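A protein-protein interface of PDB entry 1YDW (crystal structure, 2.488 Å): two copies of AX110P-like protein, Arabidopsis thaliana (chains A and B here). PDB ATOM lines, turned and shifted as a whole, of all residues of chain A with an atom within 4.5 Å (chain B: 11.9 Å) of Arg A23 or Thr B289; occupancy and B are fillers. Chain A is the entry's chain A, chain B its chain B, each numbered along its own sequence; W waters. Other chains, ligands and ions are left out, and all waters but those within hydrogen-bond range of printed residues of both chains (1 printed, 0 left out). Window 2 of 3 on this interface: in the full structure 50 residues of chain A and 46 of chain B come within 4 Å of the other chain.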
ATOM      1  N   ARG A  19     -30.495   5.143  -1.781  1.00  0.00           N
ATOM      2  CA  ARG A  19     -30.976   5.031  -3.147  1.00  0.00           C
ATOM      3  C   ARG A  19     -30.834   3.602  -3.689  1.00  0.00           C
ATOM      4  O   ARG A  19     -31.645   3.156  -4.494  1.00  0.00           O
ATOM      5  CB  ARG A  19     -30.267   6.022  -4.087  1.00  0.00           C
ATOM      6  CG  ARG A  19     -30.354   7.501  -3.665  1.00  0.00           C
ATOM      7  CD  ARG A  19     -29.801   8.486  -4.724  1.00  0.00           C
ATOM      8  NE  ARG A  19     -28.345   8.366  -4.921  1.00  0.00           N
ATOM      9  CZ  ARG A  19     -27.775   7.992  -6.070  1.00  0.00           C
ATOM     10  NH1 ARG A  19     -28.525   7.746  -7.128  1.00  0.00           N
ATOM     11  NH2 ARG A  19     -26.459   7.896  -6.180  1.00  0.00           N
ATOM     12  N   LYS A  20     -29.791   2.882  -3.294  1.00  0.00           N
ATOM     13  CA  LYS A  20     -29.589   1.520  -3.829  1.00  0.00           C
ATOM     14  C   LYS A  20     -30.346   0.552  -2.926  1.00  0.00           C
ATOM     15  O   LYS A  20     -30.905  -0.453  -3.384  1.00  0.00           O
ATOM     16  CB  LYS A  20     -28.087   1.194  -3.863  1.00  0.00           C
ATOM     17  CG  LYS A  20     -27.701  -0.247  -3.984  1.00  0.00           C
ATOM     18  CD  LYS A  20     -26.214  -0.437  -3.838  1.00  0.00           C
ATOM     19  CE  LYS A  20     -25.743  -1.844  -4.244  1.00  0.00           C
ATOM     20  NZ  LYS A  20     -24.523  -2.173  -3.474  1.00  0.00           N
ATOM     21  N   VAL A  21     -30.411   0.868  -1.637  1.00  0.00           N
ATOM     22  CA  VAL A  21     -31.284   0.041  -0.817  1.00  0.00           C
ATOM     23  C   VAL A  21     -32.811   0.133  -1.109  1.00  0.00           C
ATOM     24  O   VAL A  21     -33.504  -0.864  -0.975  1.00  0.00           O
ATOM     25  CB  VAL A  21     -30.999   0.171   0.611  1.00  0.00           C
ATOM     26  CG1 VAL A  21     -31.869  -0.802   1.371  1.00  0.00           C
ATOM     27  CG2 VAL A  21     -29.518  -0.098   0.838  1.00  0.00           C
ATOM     28  N   SER A  22     -33.309   1.281  -1.554  1.00  0.00           N
ATOM     29  CA  SER A  22     -34.720   1.401  -1.953  1.00  0.00           C
ATOM     30  C   SER A  22     -35.013   0.455  -3.075  1.00  0.00           C
ATOM     31  O   SER A  22     -36.031  -0.287  -3.012  1.00  0.00           O
ATOM     32  CB  SER A  22     -35.067   2.821  -2.353  1.00  0.00           C
ATOM     33  OG  SER A  22     -34.688   3.643  -1.285  1.00  0.00           O
ATOM     34  N   ARG A  23     -34.127   0.446  -4.089  1.00  0.00           N
ATOM     35  CA  ARG A  23     -34.172  -0.613  -5.110  1.00  0.00           C
ATOM     36  C   ARG A  23     -34.101  -2.043  -4.515  1.00  0.00           C
ATOM     37  O   ARG A  23     -34.800  -2.945  -4.989  1.00  0.00           O
ATOM     38  CB  ARG A  23     -33.147  -0.420  -6.237  1.00  0.00           C
ATOM     39  CG  ARG A  23     -33.339  -1.477  -7.342  1.00  0.00           C
ATOM     40  CD  ARG A  23     -32.912  -1.012  -8.728  1.00  0.00           C
ATOM     41  NE  ARG A  23     -31.549  -1.408  -8.931  1.00  0.00           N
ATOM     42  CZ  ARG A  23     -31.171  -2.469  -9.623  1.00  0.00           C
ATOM     43  NH1 ARG A  23     -32.056  -3.218 -10.240  1.00  0.00           N
ATOM     44  NH2 ARG A  23     -29.895  -2.770  -9.695  1.00  0.00           N
ATOM     45  N   ALA A  24     -33.289  -2.236  -3.471  1.00  0.00           N
ATOM     46  CA  ALA A  24     -33.183  -3.576  -2.837  1.00  0.00           C
ATOM     47  C   ALA A  24     -34.589  -3.954  -2.389  1.00  0.00           C
ATOM     48  O   ALA A  24     -35.221  -4.806  -2.984  1.00  0.00           O
ATOM     49  CB  ALA A  24     -32.262  -3.561  -1.648  1.00  0.00           C
ATOM     50  N   ILE A  25     -35.067  -3.270  -1.351  1.00  0.00           N
ATOM     51  CA  ILE A  25     -36.455  -3.294  -0.943  1.00  0.00           C
ATOM     52  C   ILE A  25     -37.414  -3.458  -2.121  1.00  0.00           C
ATOM     53  O   ILE A  25     -38.150  -4.429  -2.170  1.00  0.00           O
ATOM     54  CB  ILE A  25     -36.812  -2.035  -0.188  1.00  0.00           C
ATOM     55  CG1 ILE A  25     -35.997  -1.931   1.095  1.00  0.00           C
ATOM     56  CG2 ILE A  25     -38.284  -2.075   0.175  1.00  0.00           C
ATOM     57  CD1 ILE A  25     -36.242  -0.683   1.876  1.00  0.00           C
ATOM     58  N   HIS A  26     -37.398  -2.542  -3.080  1.00  0.00           N
ATOM     59  CA  HIS A  26     -38.319  -2.678  -4.200  1.00  0.00           C
ATOM     60  C   HIS A  26     -38.368  -4.115  -4.749  1.00  0.00           C
ATOM     61  O   HIS A  26     -39.392  -4.800  -4.675  1.00  0.00           O
ATOM     62  CB  HIS A  26     -37.963  -1.681  -5.300  1.00  0.00           C
ATOM     63  CG  HIS A  26     -38.904  -1.705  -6.471  1.00  0.00           C
ATOM     64  ND1 HIS A  26     -38.465  -1.710  -7.782  1.00  0.00           N
ATOM     65  CD2 HIS A  26     -40.259  -1.741  -6.531  1.00  0.00           C
ATOM     66  CE1 HIS A  26     -39.508  -1.738  -8.597  1.00  0.00           C
ATOM     67  NE2 HIS A  26     -40.607  -1.755  -7.864  1.00  0.00           N
ATOM     68  N   LEU A  27     -37.228  -4.564  -5.259  1.00  0.00           N
ATOM     69  CA  LEU A  27     -37.064  -5.867  -5.894  1.00  0.00           C
ATOM     70  C   LEU A  27     -37.277  -7.059  -4.955  1.00  0.00           C
ATOM     71  O   LEU A  27     -37.519  -8.184  -5.403  1.00  0.00           O
ATOM     72  CB  LEU A  27     -35.654  -5.935  -6.496  1.00  0.00           C
ATOM     73  CG  LEU A  27     -35.271  -4.917  -7.593  1.00  0.00           C
ATOM     74  CD1 LEU A  27     -33.775  -4.986  -7.929  1.00  0.00           C
ATOM     75  CD2 LEU A  27     -36.102  -5.072  -8.866  1.00  0.00           C
ATOM     76  N   PRO A 268     -19.868  -7.179  -6.785  1.00  0.00           N
ATOM     77  CA  PRO A 268     -19.398  -7.809  -8.013  1.00  0.00           C
ATOM     78  C   PRO A 268     -19.375  -6.868  -9.183  1.00  0.00           C
ATOM     79  O   PRO A 268     -19.973  -5.793  -9.127  1.00  0.00           O
ATOM     80  CB  PRO A 268     -20.402  -8.943  -8.263  1.00  0.00           C
ATOM     81  CG  PRO A 268     -21.536  -8.679  -7.384  1.00  0.00           C
ATOM     82  CD  PRO A 268     -21.047  -7.838  -6.227  1.00  0.00           C
ATOM     83  N   LYS A 270     -20.637  -7.106 -12.135  1.00  0.00           N
ATOM     84  CA  LYS A 270     -21.999  -6.998 -12.715  1.00  0.00           C
ATOM     85  C   LYS A 270     -22.986  -7.567 -11.696  1.00  0.00           C
ATOM     86  O   LYS A 270     -22.654  -8.543 -11.040  1.00  0.00           O
ATOM     87  CB  LYS A 270     -22.092  -7.805 -14.017  1.00  0.00           C
ATOM     88  CG  LYS A 270     -21.290  -7.158 -15.125  1.00  0.00           C
ATOM     89  CD  LYS A 270     -21.754  -7.530 -16.514  1.00  0.00           C
ATOM     90  CE  LYS A 270     -21.673  -9.020 -16.774  1.00  0.00           C
ATOM     91  NZ  LYS A 270     -21.312  -9.241 -18.208  1.00  0.00           N
ATOM     92  N   GLU A 271     -24.176  -6.993 -11.524  1.00  0.00           N
ATOM     93  CA  GLU A 271     -25.049  -7.479 -10.436  1.00  0.00           C
ATOM     94  C   GLU A 271     -25.718  -8.807 -10.792  1.00  0.00           C
ATOM     95  O   GLU A 271     -26.290  -9.458  -9.934  1.00  0.00           O
ATOM     96  CB  GLU A 271     -26.117  -6.470 -10.082  1.00  0.00           C
ATOM     97  CG  GLU A 271     -27.126  -6.195 -11.221  1.00  0.00           C
ATOM     98  CD  GLU A 271     -28.216  -5.241 -10.783  1.00  0.00           C
ATOM     99  OE1 GLU A 271     -29.094  -4.861 -11.614  1.00  0.00           O
ATOM    100  OE2 GLU A 271     -28.155  -4.867  -9.596  1.00  0.00           O
ATOM    101  N   GLU A 307     -28.094  -6.992  -2.485  1.00  0.00           N
ATOM    102  CA  GLU A 307     -28.811  -6.099  -1.564  1.00  0.00           C
ATOM    103  C   GLU A 307     -30.271  -6.511  -1.523  1.00  0.00           C
ATOM    104  O   GLU A 307     -30.856  -6.579  -0.451  1.00  0.00           O
ATOM    105  CB  GLU A 307     -28.709  -4.646  -1.954  1.00  0.00           C
ATOM    106  CG  GLU A 307     -29.170  -4.390  -3.373  1.00  0.00           C
ATOM    107  CD  GLU A 307     -28.081  -4.664  -4.405  1.00  0.00           C
ATOM    108  OE1 GLU A 307     -27.244  -5.590  -4.212  1.00  0.00           O
ATOM    109  OE2 GLU A 307     -28.058  -3.957  -5.424  1.00  0.00           O
ATOM    110  N   TRP B 283     -13.924   2.252 -10.728  1.00  0.00           N
ATOM    111  CA  TRP B 283     -15.058   2.834 -10.015  1.00  0.00           C
ATOM    112  C   TRP B 283     -16.350   2.169 -10.367  1.00  0.00           C
ATOM    113  O   TRP B 283     -16.393   1.232 -11.163  1.00  0.00           O
ATOM    114  CB  TRP B 283     -15.138   4.356 -10.252  1.00  0.00           C
ATOM    115  CG  TRP B 283     -15.800   5.114  -9.084  1.00  0.00           C
ATOM    116  CD1 TRP B 283     -16.875   5.973  -9.164  1.00  0.00           C
ATOM    117  CD2 TRP B 283     -15.462   5.035  -7.674  1.00  0.00           C
ATOM    118  NE1 TRP B 283     -17.202   6.440  -7.909  1.00  0.00           N
ATOM    119  CE2 TRP B 283     -16.356   5.890  -6.981  1.00  0.00           C
ATOM    120  CE3 TRP B 283     -14.460   4.364  -6.944  1.00  0.00           C
ATOM    121  CZ2 TRP B 283     -16.297   6.076  -5.603  1.00  0.00           C
ATOM    122  CZ3 TRP B 283     -14.408   4.540  -5.583  1.00  0.00           C
ATOM    123  CH2 TRP B 283     -15.330   5.386  -4.916  1.00  0.00           C
ATOM    124  N   PHE B 284     -17.410   2.670  -9.753  1.00  0.00           N
ATOM    125  CA  PHE B 284     -18.754   2.138  -9.936  1.00  0.00           C
ATOM    126  C   PHE B 284     -19.664   3.102 -10.726  1.00  0.00           C
ATOM    127  O   PHE B 284     -19.445   4.323 -10.714  1.00  0.00           O
ATOM    128  CB  PHE B 284     -19.369   1.892  -8.580  1.00  0.00           C
ATOM    129  CG  PHE B 284     -18.433   1.313  -7.554  1.00  0.00           C
ATOM    130  CD1 PHE B 284     -18.261  -0.058  -7.447  1.00  0.00           C
ATOM    131  CD2 PHE B 284     -17.801   2.129  -6.636  1.00  0.00           C
ATOM    132  CE1 PHE B 284     -17.473  -0.614  -6.450  1.00  0.00           C
ATOM    133  CE2 PHE B 284     -16.971   1.569  -5.618  1.00  0.00           C
ATOM    134  CZ  PHE B 284     -16.823   0.193  -5.532  1.00  0.00           C
ATOM    135  N   ASN B 285     -20.652   2.557 -11.434  1.00  0.00           N
ATOM    136  CA  ASN B 285     -21.708   3.408 -11.993  1.00  0.00           C
ATOM    137  C   ASN B 285     -22.398   4.158 -10.851  1.00  0.00           C
ATOM    138  O   ASN B 285     -22.200   3.833  -9.666  1.00  0.00           O
ATOM    139  CB  ASN B 285     -22.765   2.566 -12.730  1.00  0.00           C
ATOM    140  CG  ASN B 285     -23.311   1.466 -11.853  1.00  0.00           C
ATOM    141  OD1 ASN B 285     -23.170   1.485 -10.602  1.00  0.00           O
ATOM    142  ND2 ASN B 285     -23.907   0.477 -12.487  1.00  0.00           N
ATOM    143  N   ASP B 286     -23.240   5.125 -11.215  1.00  0.00           N
ATOM    144  CA  ASP B 286     -23.876   6.015 -10.225  1.00  0.00           C
ATOM    145  C   ASP B 286     -24.541   5.280  -9.054  1.00  0.00           C
ATOM    146  O   ASP B 286     -24.557   5.794  -7.946  1.00  0.00           O
ATOM    147  CB  ASP B 286     -24.861   6.999 -10.896  1.00  0.00           C
ATOM    148  CG  ASP B 286     -25.845   7.583  -9.900  1.00  0.00           C
ATOM    149  OD1 ASP B 286     -25.448   8.496  -9.146  1.00  0.00           O
ATOM    150  OD2 ASP B 286     -26.996   7.080  -9.825  1.00  0.00           O
ATOM    151  N   LEU B 287     -25.057   4.074  -9.294  1.00  0.00           N
ATOM    152  CA  LEU B 287     -25.837   3.354  -8.269  1.00  0.00           C
ATOM    153  C   LEU B 287     -25.084   2.237  -7.502  1.00  0.00           C
ATOM    154  O   LEU B 287     -25.675   1.549  -6.646  1.00  0.00           O
ATOM    155  CB  LEU B 287     -27.103   2.793  -8.901  1.00  0.00           C
ATOM    156  CG  LEU B 287     -28.403   2.812  -8.092  1.00  0.00           C
ATOM    157  CD1 LEU B 287     -28.485   3.916  -7.041  1.00  0.00           C
ATOM    158  CD2 LEU B 287     -29.580   2.905  -9.049  1.00  0.00           C
ATOM    159  N   VAL B 288     -23.781   2.091  -7.775  1.00  0.00           N
ATOM    160  CA  VAL B 288     -22.942   1.016  -7.206  1.00  0.00           C
ATOM    161  C   VAL B 288     -23.544  -0.391  -7.439  1.00  0.00           C
ATOM    162  O   VAL B 288     -23.506  -1.230  -6.555  1.00  0.00           O
ATOM    163  CB  VAL B 288     -22.586   1.272  -5.703  1.00  0.00           C
ATOM    164  CG1 VAL B 288     -21.473   0.403  -5.260  1.00  0.00           C
ATOM    165  CG2 VAL B 288     -22.226   2.796  -5.403  1.00  0.00           C
ATOM    166  N   THR B 289     -24.116  -0.629  -8.625  1.00  0.00           N
ATOM    167  CA  THR B 289     -24.602  -1.961  -8.987  1.00  0.00           C
ATOM    168  C   THR B 289     -23.643  -2.687  -9.928  1.00  0.00           C
ATOM    169  O   THR B 289     -23.817  -3.890 -10.236  1.00  0.00           O
ATOM    170  CB  THR B 289     -26.062  -1.936  -9.655  1.00  0.00           C
ATOM    171  OG1 THR B 289     -26.075  -1.112 -10.832  1.00  0.00           O
ATOM    172  CG2 THR B 289     -27.084  -1.424  -8.670  1.00  0.00           C
ATOM    173  N   ALA B 290     -22.652  -1.932 -10.397  1.00  0.00           N
ATOM    174  CA  ALA B 290     -21.601  -2.433 -11.273  1.00  0.00           C
ATOM    175  C   ALA B 290     -20.327  -1.577 -11.128  1.00  0.00           C
ATOM    176  O   ALA B 290     -20.445  -0.368 -10.809  1.00  0.00           O
ATOM    177  CB  ALA B 290     -22.100  -2.437 -12.744  1.00  0.00           C
ATOM    178  N   TRP B 291     -19.136  -2.196 -11.327  1.00  0.00           N
ATOM    179  CA  TRP B 291     -17.899  -1.441 -11.687  1.00  0.00           C
ATOM    180  C   TRP B 291     -18.085  -0.922 -13.093  1.00  0.00           C
ATOM    181  O   TRP B 291     -18.608  -1.636 -13.903  1.00  0.00           O
ATOM    182  CB  TRP B 291     -16.701  -2.345 -11.809  1.00  0.00           C
ATOM    183  CG  TRP B 291     -16.217  -2.996 -10.574  1.00  0.00           C
ATOM    184  CD1 TRP B 291     -16.962  -3.687  -9.661  1.00  0.00           C
ATOM    185  CD2 TRP B 291     -14.851  -3.117 -10.155  1.00  0.00           C
ATOM    186  NE1 TRP B 291     -16.154  -4.174  -8.676  1.00  0.00           N
ATOM    187  CE2 TRP B 291     -14.853  -3.858  -8.948  1.00  0.00           C
ATOM    188  CE3 TRP B 291     -13.623  -2.646 -10.669  1.00  0.00           C
ATOM    189  CZ2 TRP B 291     -13.676  -4.161  -8.234  1.00  0.00           C
ATOM    190  CZ3 TRP B 291     -12.434  -2.918  -9.939  1.00  0.00           C
ATOM    191  CH2 TRP B 291     -12.470  -3.680  -8.733  1.00  0.00           C
ATOM    192  N   VAL B 292     -17.606   0.285 -13.408  1.00  0.00           N
ATOM    193  CA  VAL B 292     -17.701   0.813 -14.803  1.00  0.00           C
ATOM    194  C   VAL B 292     -16.765   0.106 -15.792  1.00  0.00           C
ATOM    195  O   VAL B 292     -17.063   0.002 -17.009  1.00  0.00           O
ATOM    196  CB  VAL B 292     -17.604   2.368 -14.886  1.00  0.00           C
ATOM    197  CG1 VAL B 292     -17.104   2.968 -13.590  1.00  0.00           C
ATOM    198  CG2 VAL B 292     -16.813   2.839 -16.102  1.00  0.00           C
ATOM    199  N   SER B 293     -15.660  -0.413 -15.232  1.00  0.00           N
ATOM    200  CA  SER B 293     -14.619  -1.133 -15.961  1.00  0.00           C
ATOM    201  C   SER B 293     -13.820  -2.117 -15.090  1.00  0.00           C
ATOM    202  O   SER B 293     -12.984  -1.705 -14.299  1.00  0.00           O
ATOM    203  CB  SER B 293     -13.669  -0.125 -16.562  1.00  0.00           C
ATOM    204  OG  SER B 293     -13.608  -0.366 -17.949  1.00  0.00           O
ATOM    205  N   PRO B 294     -14.046  -3.421 -15.266  1.00  0.00           N
ATOM    206  CA  PRO B 294     -13.216  -4.435 -14.642  1.00  0.00           C
ATOM    207  C   PRO B 294     -11.707  -4.352 -15.039  1.00  0.00           C
ATOM    208  O   PRO B 294     -11.331  -3.719 -16.030  1.00  0.00           O
ATOM    209  CB  PRO B 294     -13.830  -5.751 -15.134  1.00  0.00           C
ATOM    210  CG  PRO B 294     -14.591  -5.398 -16.344  1.00  0.00           C
ATOM    211  CD  PRO B 294     -15.097  -4.012 -16.105  1.00  0.00           C
HETATM  212  O   HOH W   1     -22.421  -5.711  -8.736  1.00  0.00           O
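The side-chain carboxylate (OD2) of Asp B286 is in salt-bridge range of the guanidinium group (NH1) of Arg A19, at 3.2 Å. The side-chain amino group of Lys A20 lies close to the backbone carbonyl oxygen of Val B288, 3.4 Å away. The backbone carbonyl oxygen (O) of Thr B289 lies within hydrogen-bond range of the backbone NH (N) of Glu A271, at 3.4 Å.
The side-chain carboxylate (OE2) of Glu A271 lies within salt-bridge range of the guanidinium group (NH2) of Arg A23. OD1 of Asn B285 lies close to N of Leu B287 (3.5 Å). The backbone NH (N) of Val B288 lies within hydrogen-bond range of the side-chain amide oxygen (OD1) of Asn B285, at 3.0 Å. OD1 of Asn B285 sits at hydrogen-bond distance from N of Thr B289.
Among the printed residues, pairs that only touch across the chains: Arg A23 with Thr B289, Lys A20 with Leu B287, Pro A268 with Trp B291 and Arg A19 with Leu B287.
Of chain B, only Thr B289 (3.3 Å) comes within 4 Å of Arg A23. Of chain A, only Arg A23 and Glu A271 come within 4 Å of Thr B289. Val A21 touches none of the printed residues of chain B. No residue of chain B comes within 4 Å of Ser A22. No residue of chain B comes within 4 Å of Ile A25. His A26 touches none of the printed residues of chain B. Glu A271 touches just one residue of chain B: Thr B289. Of the printed residues of chain A, Leu B287 touches Arg A19 (3.8 Å) and Lys A20 (3.5 Å). Of the printed residues of chain A, Val B288 touches Lys A20 (3.3 Å). Of the printed residues of chain A, Trp B291 touches Pro A268. The nearest residue of chain B that does not touch Arg A23 is Leu B287 (4.7 Å).
Hydrophobic or aromatic side chains of chain B within 4 Å of the printed part of chain A: Leu B287 and Trp B291. Of the 13 printed residues of chain A, 5 touch a printed residue of chain B. Along chain A the printed residues that touch a printed residue of chain B span positions 19 to 271. Among the printed residues, 7 pairs touch across the chains.
No position is printed for both chains.
Water W1 lies within hydrogen-bond range of O of Pro A268 (2.5 Å) and O of Thr B289 (2.7 Å).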
